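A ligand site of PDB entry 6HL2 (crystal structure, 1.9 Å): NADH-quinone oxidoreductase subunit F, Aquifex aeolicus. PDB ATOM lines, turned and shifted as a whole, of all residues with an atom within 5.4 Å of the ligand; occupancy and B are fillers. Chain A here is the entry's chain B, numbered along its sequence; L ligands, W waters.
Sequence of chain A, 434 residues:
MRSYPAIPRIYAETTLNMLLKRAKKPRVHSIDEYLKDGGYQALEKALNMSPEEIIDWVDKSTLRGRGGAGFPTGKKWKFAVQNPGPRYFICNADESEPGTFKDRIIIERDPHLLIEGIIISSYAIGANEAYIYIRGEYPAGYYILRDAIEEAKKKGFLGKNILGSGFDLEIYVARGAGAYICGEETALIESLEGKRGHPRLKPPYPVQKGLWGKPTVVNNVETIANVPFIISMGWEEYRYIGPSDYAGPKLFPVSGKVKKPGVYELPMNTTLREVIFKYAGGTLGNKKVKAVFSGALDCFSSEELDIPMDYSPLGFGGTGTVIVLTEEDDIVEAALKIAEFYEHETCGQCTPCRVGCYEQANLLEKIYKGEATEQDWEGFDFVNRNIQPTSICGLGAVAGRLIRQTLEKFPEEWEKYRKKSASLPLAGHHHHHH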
ATOM      1  N   GLY A  65      14.603 -23.970  19.258  1.00  0.00           N
ATOM      2  CA  GLY A  65      14.928 -23.473  20.589  1.00  0.00           C
ATOM      3  C   GLY A  65      14.913 -21.969  20.690  1.00  0.00           C
ATOM      4  O   GLY A  65      15.385 -21.283  19.778  1.00  0.00           O
ATOM      5  N   ARG A  66      14.329 -21.450  21.782  1.00  0.00           N
ATOM      6  CA  ARG A  66      14.176 -20.005  22.023  1.00  0.00           C
ATOM      7  C   ARG A  66      15.263 -19.417  22.948  1.00  0.00           C
ATOM      8  O   ARG A  66      15.236 -18.205  23.213  1.00  0.00           O
ATOM      9  CB  ARG A  66      12.781 -19.716  22.617  1.00  0.00           C
ATOM     10  CG  ARG A  66      11.583 -20.163  21.769  1.00  0.00           C
ATOM     11  CD  ARG A  66      11.514 -19.404  20.460  1.00  0.00           C
ATOM     12  NE  ARG A  66      10.200 -19.496  19.828  1.00  0.00           N
ATOM     13  CZ  ARG A  66       9.978 -20.047  18.646  1.00  0.00           C
ATOM     14  NH1 ARG A  66       8.760 -20.057  18.124  1.00  0.00           N
ATOM     15  NH2 ARG A  66      10.973 -20.611  17.970  1.00  0.00           N
ATOM     16  N   GLY A  67      16.181 -20.248  23.420  1.00  0.00           N
ATOM     17  CA  GLY A  67      17.266 -19.850  24.314  1.00  0.00           C
ATOM     18  C   GLY A  67      18.466 -19.175  23.671  1.00  0.00           C
ATOM     19  O   GLY A  67      19.369 -18.758  24.390  1.00  0.00           O
ATOM     20  N   GLY A  68      18.509 -19.067  22.341  1.00  0.00           N
ATOM     21  CA  GLY A  68      19.611 -18.397  21.664  1.00  0.00           C
ATOM     22  C   GLY A  68      20.331 -19.183  20.583  1.00  0.00           C
ATOM     23  O   GLY A  68      20.805 -18.591  19.609  1.00  0.00           O
ATOM     24  N   ALA A  69      20.437 -20.522  20.738  1.00  0.00           N
ATOM     25  CA  ALA A  69      21.142 -21.338  19.754  1.00  0.00           C
ATOM     26  C   ALA A  69      20.248 -21.836  18.603  1.00  0.00           C
ATOM     27  O   ALA A  69      20.750 -22.298  17.577  1.00  0.00           O
ATOM     28  CB  ALA A  69      21.855 -22.516  20.454  1.00  0.00           C
ATOM     29  N   GLY A  70      18.929 -21.755  18.794  1.00  0.00           N
ATOM     30  CA  GLY A  70      17.940 -22.118  17.784  1.00  0.00           C
ATOM     31  C   GLY A  70      17.986 -23.533  17.236  1.00  0.00           C
ATOM     32  O   GLY A  70      17.658 -23.752  16.061  1.00  0.00           O
ATOM     33  N   PHE A  71      18.365 -24.530  18.078  1.00  0.00           N
ATOM     34  CA  PHE A  71      18.427 -25.914  17.626  1.00  0.00           C
ATOM     35  C   PHE A  71      16.995 -26.487  17.470  1.00  0.00           C
ATOM     36  O   PHE A  71      16.157 -26.255  18.335  1.00  0.00           O
ATOM     37  CB  PHE A  71      19.272 -26.785  18.584  1.00  0.00           C
ATOM     38  CG  PHE A  71      19.620 -28.147  18.027  1.00  0.00           C
ATOM     39  CD1 PHE A  71      18.795 -29.240  18.233  1.00  0.00           C
ATOM     40  CD2 PHE A  71      20.784 -28.331  17.278  1.00  0.00           C
ATOM     41  CE1 PHE A  71      19.105 -30.497  17.683  1.00  0.00           C
ATOM     42  CE2 PHE A  71      21.111 -29.591  16.771  1.00  0.00           C
ATOM     43  CZ  PHE A  71      20.267 -30.666  16.961  1.00  0.00           C
ATOM     44  N   THR A  73      13.876 -28.383  18.123  1.00  0.00           N
ATOM     45  CA  THR A  73      13.440 -29.043  19.359  1.00  0.00           C
ATOM     46  C   THR A  73      13.167 -30.532  19.201  1.00  0.00           C
ATOM     47  O   THR A  73      13.680 -31.327  19.995  1.00  0.00           O
ATOM     48  CB  THR A  73      12.260 -28.283  19.975  1.00  0.00           C
ATOM     49  OG1 THR A  73      12.625 -26.909  20.038  1.00  0.00           O
ATOM     50  CG2 THR A  73      11.888 -28.790  21.365  1.00  0.00           C
ATOM     51  N   LYS A  76      16.373 -32.380  18.832  1.00  0.00           N
ATOM     52  CA  LYS A  76      17.083 -32.497  20.105  1.00  0.00           C
ATOM     53  C   LYS A  76      16.520 -33.685  20.904  1.00  0.00           C
ATOM     54  O   LYS A  76      17.297 -34.509  21.399  1.00  0.00           O
ATOM     55  CB  LYS A  76      16.953 -31.198  20.919  1.00  0.00           C
ATOM     56  CG  LYS A  76      17.836 -31.211  22.168  1.00  0.00           C
ATOM     57  CD  LYS A  76      17.535 -30.069  23.141  1.00  0.00           C
ATOM     58  CE  LYS A  76      17.851 -28.706  22.560  1.00  0.00           C
ATOM     59  NZ  LYS A  76      17.936 -27.652  23.599  1.00  0.00           N
ATOM     60  N   ASN A  92      15.075 -24.426  31.375  1.00  0.00           N
ATOM     61  CA  ASN A  92      16.059 -23.388  31.608  1.00  0.00           C
ATOM     62  C   ASN A  92      15.316 -22.050  31.814  1.00  0.00           C
ATOM     63  O   ASN A  92      14.858 -21.443  30.858  1.00  0.00           O
ATOM     64  CB  ASN A  92      17.065 -23.288  30.444  1.00  0.00           C
ATOM     65  CG  ASN A  92      18.245 -22.405  30.738  1.00  0.00           C
ATOM     66  OD1 ASN A  92      18.223 -21.576  31.667  1.00  0.00           O
ATOM     67  ND2 ASN A  92      19.330 -22.583  29.964  1.00  0.00           N
ATOM     68  N   ASP A  94      16.870 -19.549  33.573  1.00  0.00           N
ATOM     69  CA  ASP A  94      17.907 -18.661  34.116  1.00  0.00           C
ATOM     70  C   ASP A  94      17.812 -17.210  33.570  1.00  0.00           C
ATOM     71  O   ASP A  94      18.182 -16.272  34.278  1.00  0.00           O
ATOM     72  CB  ASP A  94      19.319 -19.227  33.960  1.00  0.00           C
ATOM     73  CG  ASP A  94      20.285 -18.560  34.905  1.00  0.00           C
ATOM     74  OD1 ASP A  94      20.136 -18.750  36.125  1.00  0.00           O
ATOM     75  OD2 ASP A  94      21.129 -17.761  34.425  1.00  0.00           O
ATOM     76  N   GLU A  95      17.290 -17.047  32.347  1.00  0.00           N
ATOM     77  CA  GLU A  95      17.149 -15.735  31.664  1.00  0.00           C
ATOM     78  C   GLU A  95      18.462 -14.906  31.863  1.00  0.00           C
ATOM     79  O   GLU A  95      19.523 -15.432  31.520  1.00  0.00           O
ATOM     80  CB  GLU A  95      15.826 -15.052  32.096  1.00  0.00           C
ATOM     81  CG  GLU A  95      15.393 -13.904  31.190  1.00  0.00           C
ATOM     82  CD  GLU A  95      13.918 -13.861  30.841  1.00  0.00           C
ATOM     83  OE1 GLU A  95      13.076 -13.709  31.764  1.00  0.00           O
ATOM     84  OE2 GLU A  95      13.612 -13.983  29.646  1.00  0.00           O
ATOM     85  N   SER A  96      18.430 -13.717  32.460  1.00  0.00           N
ATOM     86  CA  SER A  96      19.624 -12.917  32.844  1.00  0.00           C
ATOM     87  C   SER A  96      20.387 -12.166  31.736  1.00  0.00           C
ATOM     88  O   SER A  96      21.263 -11.369  32.077  1.00  0.00           O
ATOM     89  CB  SER A  96      20.628 -13.755  33.638  1.00  0.00           C
ATOM     90  OG  SER A  96      19.987 -14.285  34.786  1.00  0.00           O
ATOM     91  N   ASP A 103      10.820 -14.606  29.441  1.00  0.00           N
ATOM     92  CA  ASP A 103      10.500 -15.869  30.154  1.00  0.00           C
ATOM     93  C   ASP A 103       9.761 -15.662  31.449  1.00  0.00           C
ATOM     94  O   ASP A 103       8.836 -16.422  31.764  1.00  0.00           O
ATOM     95  CB  ASP A 103      11.759 -16.716  30.398  1.00  0.00           C
ATOM     96  CG  ASP A 103      12.462 -17.183  29.126  1.00  0.00           C
ATOM     97  OD1 ASP A 103      11.821 -17.148  28.058  1.00  0.00           O
ATOM     98  OD2 ASP A 103      13.664 -17.580  29.222  1.00  0.00           O
ATOM     99  N   TYR A 180      25.304 -15.526  35.690  1.00  0.00           N
ATOM    100  CA  TYR A 180      24.726 -15.542  34.338  1.00  0.00           C
ATOM    101  C   TYR A 180      25.155 -16.793  33.588  1.00  0.00           C
ATOM    102  O   TYR A 180      24.395 -17.326  32.767  1.00  0.00           O
ATOM    103  CB  TYR A 180      25.190 -14.297  33.553  1.00  0.00           C
ATOM    104  CG  TYR A 180      24.968 -14.360  32.063  1.00  0.00           C
ATOM    105  CD1 TYR A 180      23.704 -14.160  31.515  1.00  0.00           C
ATOM    106  CD2 TYR A 180      26.027 -14.589  31.185  1.00  0.00           C
ATOM    107  CE1 TYR A 180      23.498 -14.200  30.133  1.00  0.00           C
ATOM    108  CE2 TYR A 180      25.830 -14.618  29.812  1.00  0.00           C
ATOM    109  CZ  TYR A 180      24.565 -14.424  29.286  1.00  0.00           C
ATOM    110  OH  TYR A 180      24.389 -14.453  27.914  1.00  0.00           O
ATOM    111  N   ILE A 181      26.388 -17.256  33.852  1.00  0.00           N
ATOM    112  CA  ILE A 181      26.933 -18.435  33.215  1.00  0.00           C
ATOM    113  C   ILE A 181      26.092 -19.698  33.486  1.00  0.00           C
ATOM    114  O   ILE A 181      26.147 -20.632  32.693  1.00  0.00           O
ATOM    115  CB  ILE A 181      28.446 -18.623  33.556  1.00  0.00           C
ATOM    116  CG1 ILE A 181      29.119 -19.600  32.584  1.00  0.00           C
ATOM    117  CG2 ILE A 181      28.642 -19.086  35.023  1.00  0.00           C
ATOM    118  CD1 ILE A 181      28.985 -19.211  31.064  1.00  0.00           C
ATOM    119  N   GLY A 183      23.108 -20.161  32.952  1.00  0.00           N
ATOM    120  CA  GLY A 183      22.134 -20.321  31.890  1.00  0.00           C
ATOM    121  C   GLY A 183      22.704 -21.201  30.781  1.00  0.00           C
ATOM    122  O   GLY A 183      21.952 -21.779  29.990  1.00  0.00           O
ATOM    123  N   GLU A 184      24.068 -21.311  30.700  1.00  0.00           N
ATOM    124  CA  GLU A 184      24.723 -22.179  29.705  1.00  0.00           C
ATOM    125  C   GLU A 184      24.404 -23.590  30.153  1.00  0.00           C
ATOM    126  O   GLU A 184      24.555 -23.908  31.332  1.00  0.00           O
ATOM    127  CB  GLU A 184      26.260 -21.926  29.667  1.00  0.00           C
ATOM    128  CG  GLU A 184      26.930 -22.516  28.440  1.00  0.00           C
ATOM    129  CD  GLU A 184      27.299 -23.986  28.491  1.00  0.00           C
ATOM    130  OE1 GLU A 184      27.379 -24.539  29.614  1.00  0.00           O
ATOM    131  OE2 GLU A 184      27.571 -24.573  27.430  1.00  0.00           O
ATOM    132  N   GLU A 185      23.844 -24.390  29.254  1.00  0.00           N
ATOM    133  CA  GLU A 185      23.279 -25.712  29.611  1.00  0.00           C
ATOM    134  C   GLU A 185      24.200 -26.633  30.439  1.00  0.00           C
ATOM    135  O   GLU A 185      23.707 -27.273  31.372  1.00  0.00           O
ATOM    136  CB  GLU A 185      22.736 -26.437  28.390  1.00  0.00           C
ATOM    137  CG  GLU A 185      23.735 -26.684  27.279  1.00  0.00           C
ATOM    138  CD  GLU A 185      23.152 -27.357  26.056  1.00  0.00           C
ATOM    139  OE1 GLU A 185      21.983 -27.799  26.108  1.00  0.00           O
ATOM    140  OE2 GLU A 185      23.879 -27.464  25.046  1.00  0.00           O
ATOM    141  N   VAL A 218      17.739 -30.095  27.800  1.00  0.00           N
ATOM    142  CA  VAL A 218      17.578 -28.781  28.395  1.00  0.00           C
ATOM    143  C   VAL A 218      16.807 -27.951  27.347  1.00  0.00           C
ATOM    144  O   VAL A 218      17.231 -27.906  26.200  1.00  0.00           O
ATOM    145  CB  VAL A 218      18.933 -28.115  28.743  1.00  0.00           C
ATOM    146  CG1 VAL A 218      18.725 -26.706  29.295  1.00  0.00           C
ATOM    147  CG2 VAL A 218      19.736 -28.979  29.728  1.00  0.00           C
ATOM    148  N   ASN A 219      15.676 -27.343  27.731  1.00  0.00           N
ATOM    149  CA  ASN A 219      14.918 -26.449  26.844  1.00  0.00           C
ATOM    150  C   ASN A 219      14.582 -25.166  27.561  1.00  0.00           C
ATOM    151  O   ASN A 219      14.355 -25.171  28.780  1.00  0.00           O
ATOM    152  CB  ASN A 219      13.654 -27.091  26.280  1.00  0.00           C
ATOM    153  CG  ASN A 219      13.902 -27.911  25.032  1.00  0.00           C
ATOM    154  OD1 ASN A 219      13.538 -29.080  24.977  1.00  0.00           O
ATOM    155  ND2 ASN A 219      14.430 -27.319  23.969  1.00  0.00           N
ATOM    156  N   ASN A 220      14.581 -24.056  26.815  1.00  0.00           N
ATOM    157  CA  ASN A 220      14.253 -22.728  27.359  1.00  0.00           C
ATOM    158  C   ASN A 220      12.757 -22.677  27.681  1.00  0.00           C
ATOM    159  O   ASN A 220      11.966 -23.365  27.046  1.00  0.00           O
ATOM    160  CB  ASN A 220      14.587 -21.682  26.293  1.00  0.00           C
ATOM    161  CG  ASN A 220      14.149 -20.282  26.632  1.00  0.00           C
ATOM    162  OD1 ASN A 220      13.137 -19.812  26.131  1.00  0.00           O
ATOM    163  ND2 ASN A 220      14.825 -19.642  27.560  1.00  0.00           N
ATOM    164  N   VAL A 221      12.371 -21.855  28.678  1.00  0.00           N
ATOM    165  CA  VAL A 221      10.954 -21.618  29.067  1.00  0.00           C
ATOM    166  C   VAL A 221      10.042 -21.380  27.862  1.00  0.00           C
ATOM    167  O   VAL A 221       8.967 -21.967  27.775  1.00  0.00           O
ATOM    168  CB  VAL A 221      10.845 -20.408  30.044  1.00  0.00           C
ATOM    169  CG1 VAL A 221       9.381 -19.968  30.225  1.00  0.00           C
ATOM    170  CG2 VAL A 221      11.490 -20.737  31.370  1.00  0.00           C
ATOM    171  N   THR A 223      10.495 -22.002  24.616  1.00  0.00           N
ATOM    172  CA  THR A 223      10.410 -23.186  23.738  1.00  0.00           C
ATOM    173  C   THR A 223       9.341 -24.139  24.292  1.00  0.00           C
ATOM    174  O   THR A 223       8.449 -24.562  23.544  1.00  0.00           O
ATOM    175  CB  THR A 223      11.733 -23.950  23.701  1.00  0.00           C
ATOM    176  OG1 THR A 223      12.816 -23.033  23.514  1.00  0.00           O
ATOM    177  CG2 THR A 223      11.749 -25.056  22.626  1.00  0.00           C
ATOM    178  N   CYS A 393      32.986 -22.350  26.153  1.00  0.00           N
ATOM    179  CA  CYS A 393      31.556 -22.070  25.970  1.00  0.00           C
ATOM    180  C   CYS A 393      31.291 -20.819  25.131  1.00  0.00           C
ATOM    181  O   CYS A 393      32.219 -20.122  24.758  1.00  0.00           O
ATOM    182  CB  CYS A 393      30.833 -22.034  27.322  1.00  0.00           C
ATOM    183  SG  CYS A 393      30.738 -20.393  28.117  1.00  0.00           S
ATOM    184  N   GLY A 394      30.006 -20.563  24.847  1.00  0.00           N
ATOM    185  CA  GLY A 394      29.559 -19.447  24.029  1.00  0.00           C
ATOM    186  C   GLY A 394      29.904 -18.062  24.529  1.00  0.00           C
ATOM    187  O   GLY A 394      30.004 -17.150  23.726  1.00  0.00           O
ATOM    188  N   LEU A 395      30.045 -17.876  25.866  1.00  0.00           N
ATOM    189  CA  LEU A 395      30.346 -16.558  26.430  1.00  0.00           C
ATOM    190  C   LEU A 395      31.642 -15.940  25.865  1.00  0.00           C
ATOM    191  O   LEU A 395      31.628 -14.807  25.420  1.00  0.00           O
ATOM    192  CB  LEU A 395      30.345 -16.582  27.969  1.00  0.00           C
ATOM    193  CG  LEU A 395      30.310 -15.217  28.671  1.00  0.00           C
ATOM    194  CD1 LEU A 395      29.664 -15.333  30.039  1.00  0.00           C
ATOM    195  CD2 LEU A 395      31.742 -14.621  28.843  1.00  0.00           C
HETATM  196  N1  LIG L   1      19.380 -20.600  27.296  1.00  0.00           N
HETATM  197  C1  LIG L   1      18.287 -20.334  28.052  1.00  0.00           C
HETATM  198  O1  LIG L   1      17.244 -20.986  27.899  1.00  0.00           O
HETATM  199  N2  LIG L   1      18.372 -19.395  29.074  1.00  0.00           N
HETATM  200  C2  LIG L   1      19.506 -18.691  29.435  1.00  0.00           C
HETATM  201  O2  LIG L   1      19.472 -17.916  30.395  1.00  0.00           O
HETATM  202  C3  LIG L   1      20.679 -19.015  28.655  1.00  0.00           C
HETATM  203  N3  LIG L   1      21.822 -18.471  28.989  1.00  0.00           N
HETATM  204  C4  LIG L   1      22.961 -18.846  28.299  1.00  0.00           C
HETATM  205  C5  LIG L   1      24.183 -18.277  28.662  1.00  0.00           C
HETATM  206  C6  LIG L   1      25.343 -18.575  27.957  1.00  0.00           C
HETATM  207  C7  LIG L   1      26.645 -17.906  28.364  1.00  0.00           C
HETATM  208  C8  LIG L   1      25.292 -19.477  26.867  1.00  0.00           C
HETATM  209  C9  LIG L   1      26.517 -19.781  26.044  1.00  0.00           C
HETATM  210  C10 LIG L   1      24.078 -20.072  26.531  1.00  0.00           C
HETATM  211  C11 LIG L   1      22.908 -19.767  27.223  1.00  0.00           C
HETATM  212  N4  LIG L   1      21.654 -20.347  26.902  1.00  0.00           N
HETATM  213  C12 LIG L   1      20.525 -19.991  27.596  1.00  0.00           C
HETATM  214  C13 LIG L   1      21.606 -21.426  25.900  1.00  0.00           C
HETATM  215  C14 LIG L   1      21.598 -22.811  26.551  1.00  0.00           C
HETATM  216  O3  LIG L   1      22.934 -23.269  26.757  1.00  0.00           O
HETATM  217  C15 LIG L   1      20.792 -23.817  25.716  1.00  0.00           C
HETATM  218  O4  LIG L   1      21.178 -23.695  24.346  1.00  0.00           O
HETATM  219  C16 LIG L   1      19.268 -23.703  25.799  1.00  0.00           C
HETATM  220  O5  LIG L   1      18.836 -23.611  27.162  1.00  0.00           O
HETATM  221  C17 LIG L   1      18.603 -24.891  25.131  1.00  0.00           C
HETATM  222  O6  LIG L   1      17.168 -24.661  25.050  1.00  0.00           O
HETATM  223  P1  LIG L   1      16.435 -24.286  23.691  1.00  0.00           P
HETATM  224  O7  LIG L   1      16.774 -22.916  23.242  1.00  0.00           O
HETATM  225  O8  LIG L   1      16.850 -25.344  22.644  1.00  0.00           O
HETATM  226  O9  LIG L   1      14.956 -24.484  23.996  1.00  0.00           O
HETATM  227  O   HOH W   1      22.162 -15.655  27.007  1.00  0.00           O
HETATM  228  O   HOH W   2      15.329 -26.784  20.928  1.00  0.00           O
HETATM  229  O   HOH W   3      19.314 -22.255  22.630  1.00  0.00           O
HETATM  230  O   HOH W   4      18.855 -17.130  26.437  1.00  0.00           O
HETATM  231  O   HOH W   5      15.843 -18.758  30.466  1.00  0.00           O
HETATM  232  O   HOH W   6      21.846 -16.974  31.927  1.00  0.00           O
HETATM  233  O   HOH W   7      18.784 -24.483  20.920  1.00  0.00           O
HETATM  234  O   HOH W   8      20.453 -15.713  29.072  1.00  0.00           O
HETATM  235  O   HOH W   9      22.840 -25.571  23.383  1.00  0.00           O
HETATM  236  O   HOH W  10      23.758 -16.948  25.263  1.00  0.00           O
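The side-chain hydroxyl of Thr 223 sits at hydrogen-bond distance from an oxygen (O9) of the ligand (2.6 Å). The side-chain amino group (NZ) of Lys 76 lies within salt-bridge range of an oxygen (O8) of the ligand (2.7 Å). An oxygen (O2) of the ligand sits at hydrogen-bond distance from the backbone NH (N) of Glu 95 (3.1 Å). O of Glu 95 lies close to O2 of the ligand, at 2.7 Å. N of Gly 67 lies within hydrogen-bond range of O7 of the ligand (2.7 Å). The backbone NH of Asn 220 sits at hydrogen-bond distance from an oxygen (O9) of the ligand, at 2.9 Å. An oxygen (O1) of the ligand sits at hydrogen-bond distance from the side-chain amide nitrogen of Asn 220, at 2.8 Å. The side-chain amide nitrogen (ND2) of Asn 219 is in hydrogen-bond range of an oxygen (O9) of the ligand, at 2.9 Å. O3 of the ligand sits at hydrogen-bond distance from N of Glu 185 (2.9 Å). ND2 of Asn 92 lies within hydrogen-bond range of O5 of the ligand (3.0 Å). The backbone NH (N) of Arg 66 lies within hydrogen-bond range of an oxygen (O7) of the ligand (3.2 Å).
The side-chain amino group of Lys 76 is in hydrogen-bond range of the backbone carbonyl oxygen of Val 218 (2.7 Å). OE2 of Glu 95 is in hydrogen-bond range of N of Asp 103. ND2 of Asn 220 lies within hydrogen-bond range of OD2 of Asp 103, at 2.9 Å. The side-chain amide nitrogen (ND2) of Asn 92 is in hydrogen-bond range of the backbone carbonyl oxygen (O) of Gly 183 (2.7 Å). The backbone carbonyl oxygen of Asn 92 is in hydrogen-bond range of the backbone NH of Val 221 (3.3 Å). The backbone NH (N) of Gly 65 lies within hydrogen-bond range of the backbone carbonyl oxygen (O) of Phe 71 (2.9 Å). O of Asp 94 is in hydrogen-bond range of OG of Ser 96 (2.7 Å). The side-chain sulfur of Cys 393 sits close to the backbone NH of Leu 395 (3.4 Å).
N4 of the ligand sits close to O of Gly 183 (3.4 Å). An oxygen (O6) of the ligand sits close to the backbone carbonyl oxygen (O) of Val 218 (3.4 Å). CA of Gly 65 touches O7 of the ligand, 3.3 Å away. Asp 94 touches the ligand (C to O2, 3.7 Å). Tyr 180 touches the ligand. Ile 181 touches the ligand (CD1 to C7, 3.8 Å). N of Glu 184 touches C4 of the ligand, at 3.6 Å. CA of Gly 394 touches C9 of the ligand, at 3.7 Å. Leu 395 touches the ligand (CB to C7, 3.9 Å).
Water W9 bridges O4 of the ligand (2.7 Å) and OE2 of Glu 185 (2.7 Å). Water W3 lies within hydrogen-bond range of an oxygen (O7) of the ligand (2.7 Å), the backbone NH (N) of Ala 69 (2.8 Å) and the backbone NH (N) of Gly 68 (3.3 Å). Water W2 lies within hydrogen-bond range of O8 of the ligand (2.7 Å), O of Phe 71 (2.8 Å), OG1 of Thr 73 (2.8 Å), ND2 of Asn 219 (3.2 Å) and N of Gly 65 (3.4 Å). Water W7 lies within hydrogen-bond range of an oxygen (O8) of the ligand (2.7 Å), the backbone NH of Phe 71 (2.9 Å) and the backbone NH of Gly 70 (3.5 Å). Water W8 lies within hydrogen-bond range of the backbone carbonyl oxygen of Glu 95 and an oxygen (O2) of the ligand. Water W1 bridges the side-chain hydroxyl of Tyr 180 and a nitrogen (N3) of the ligand.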
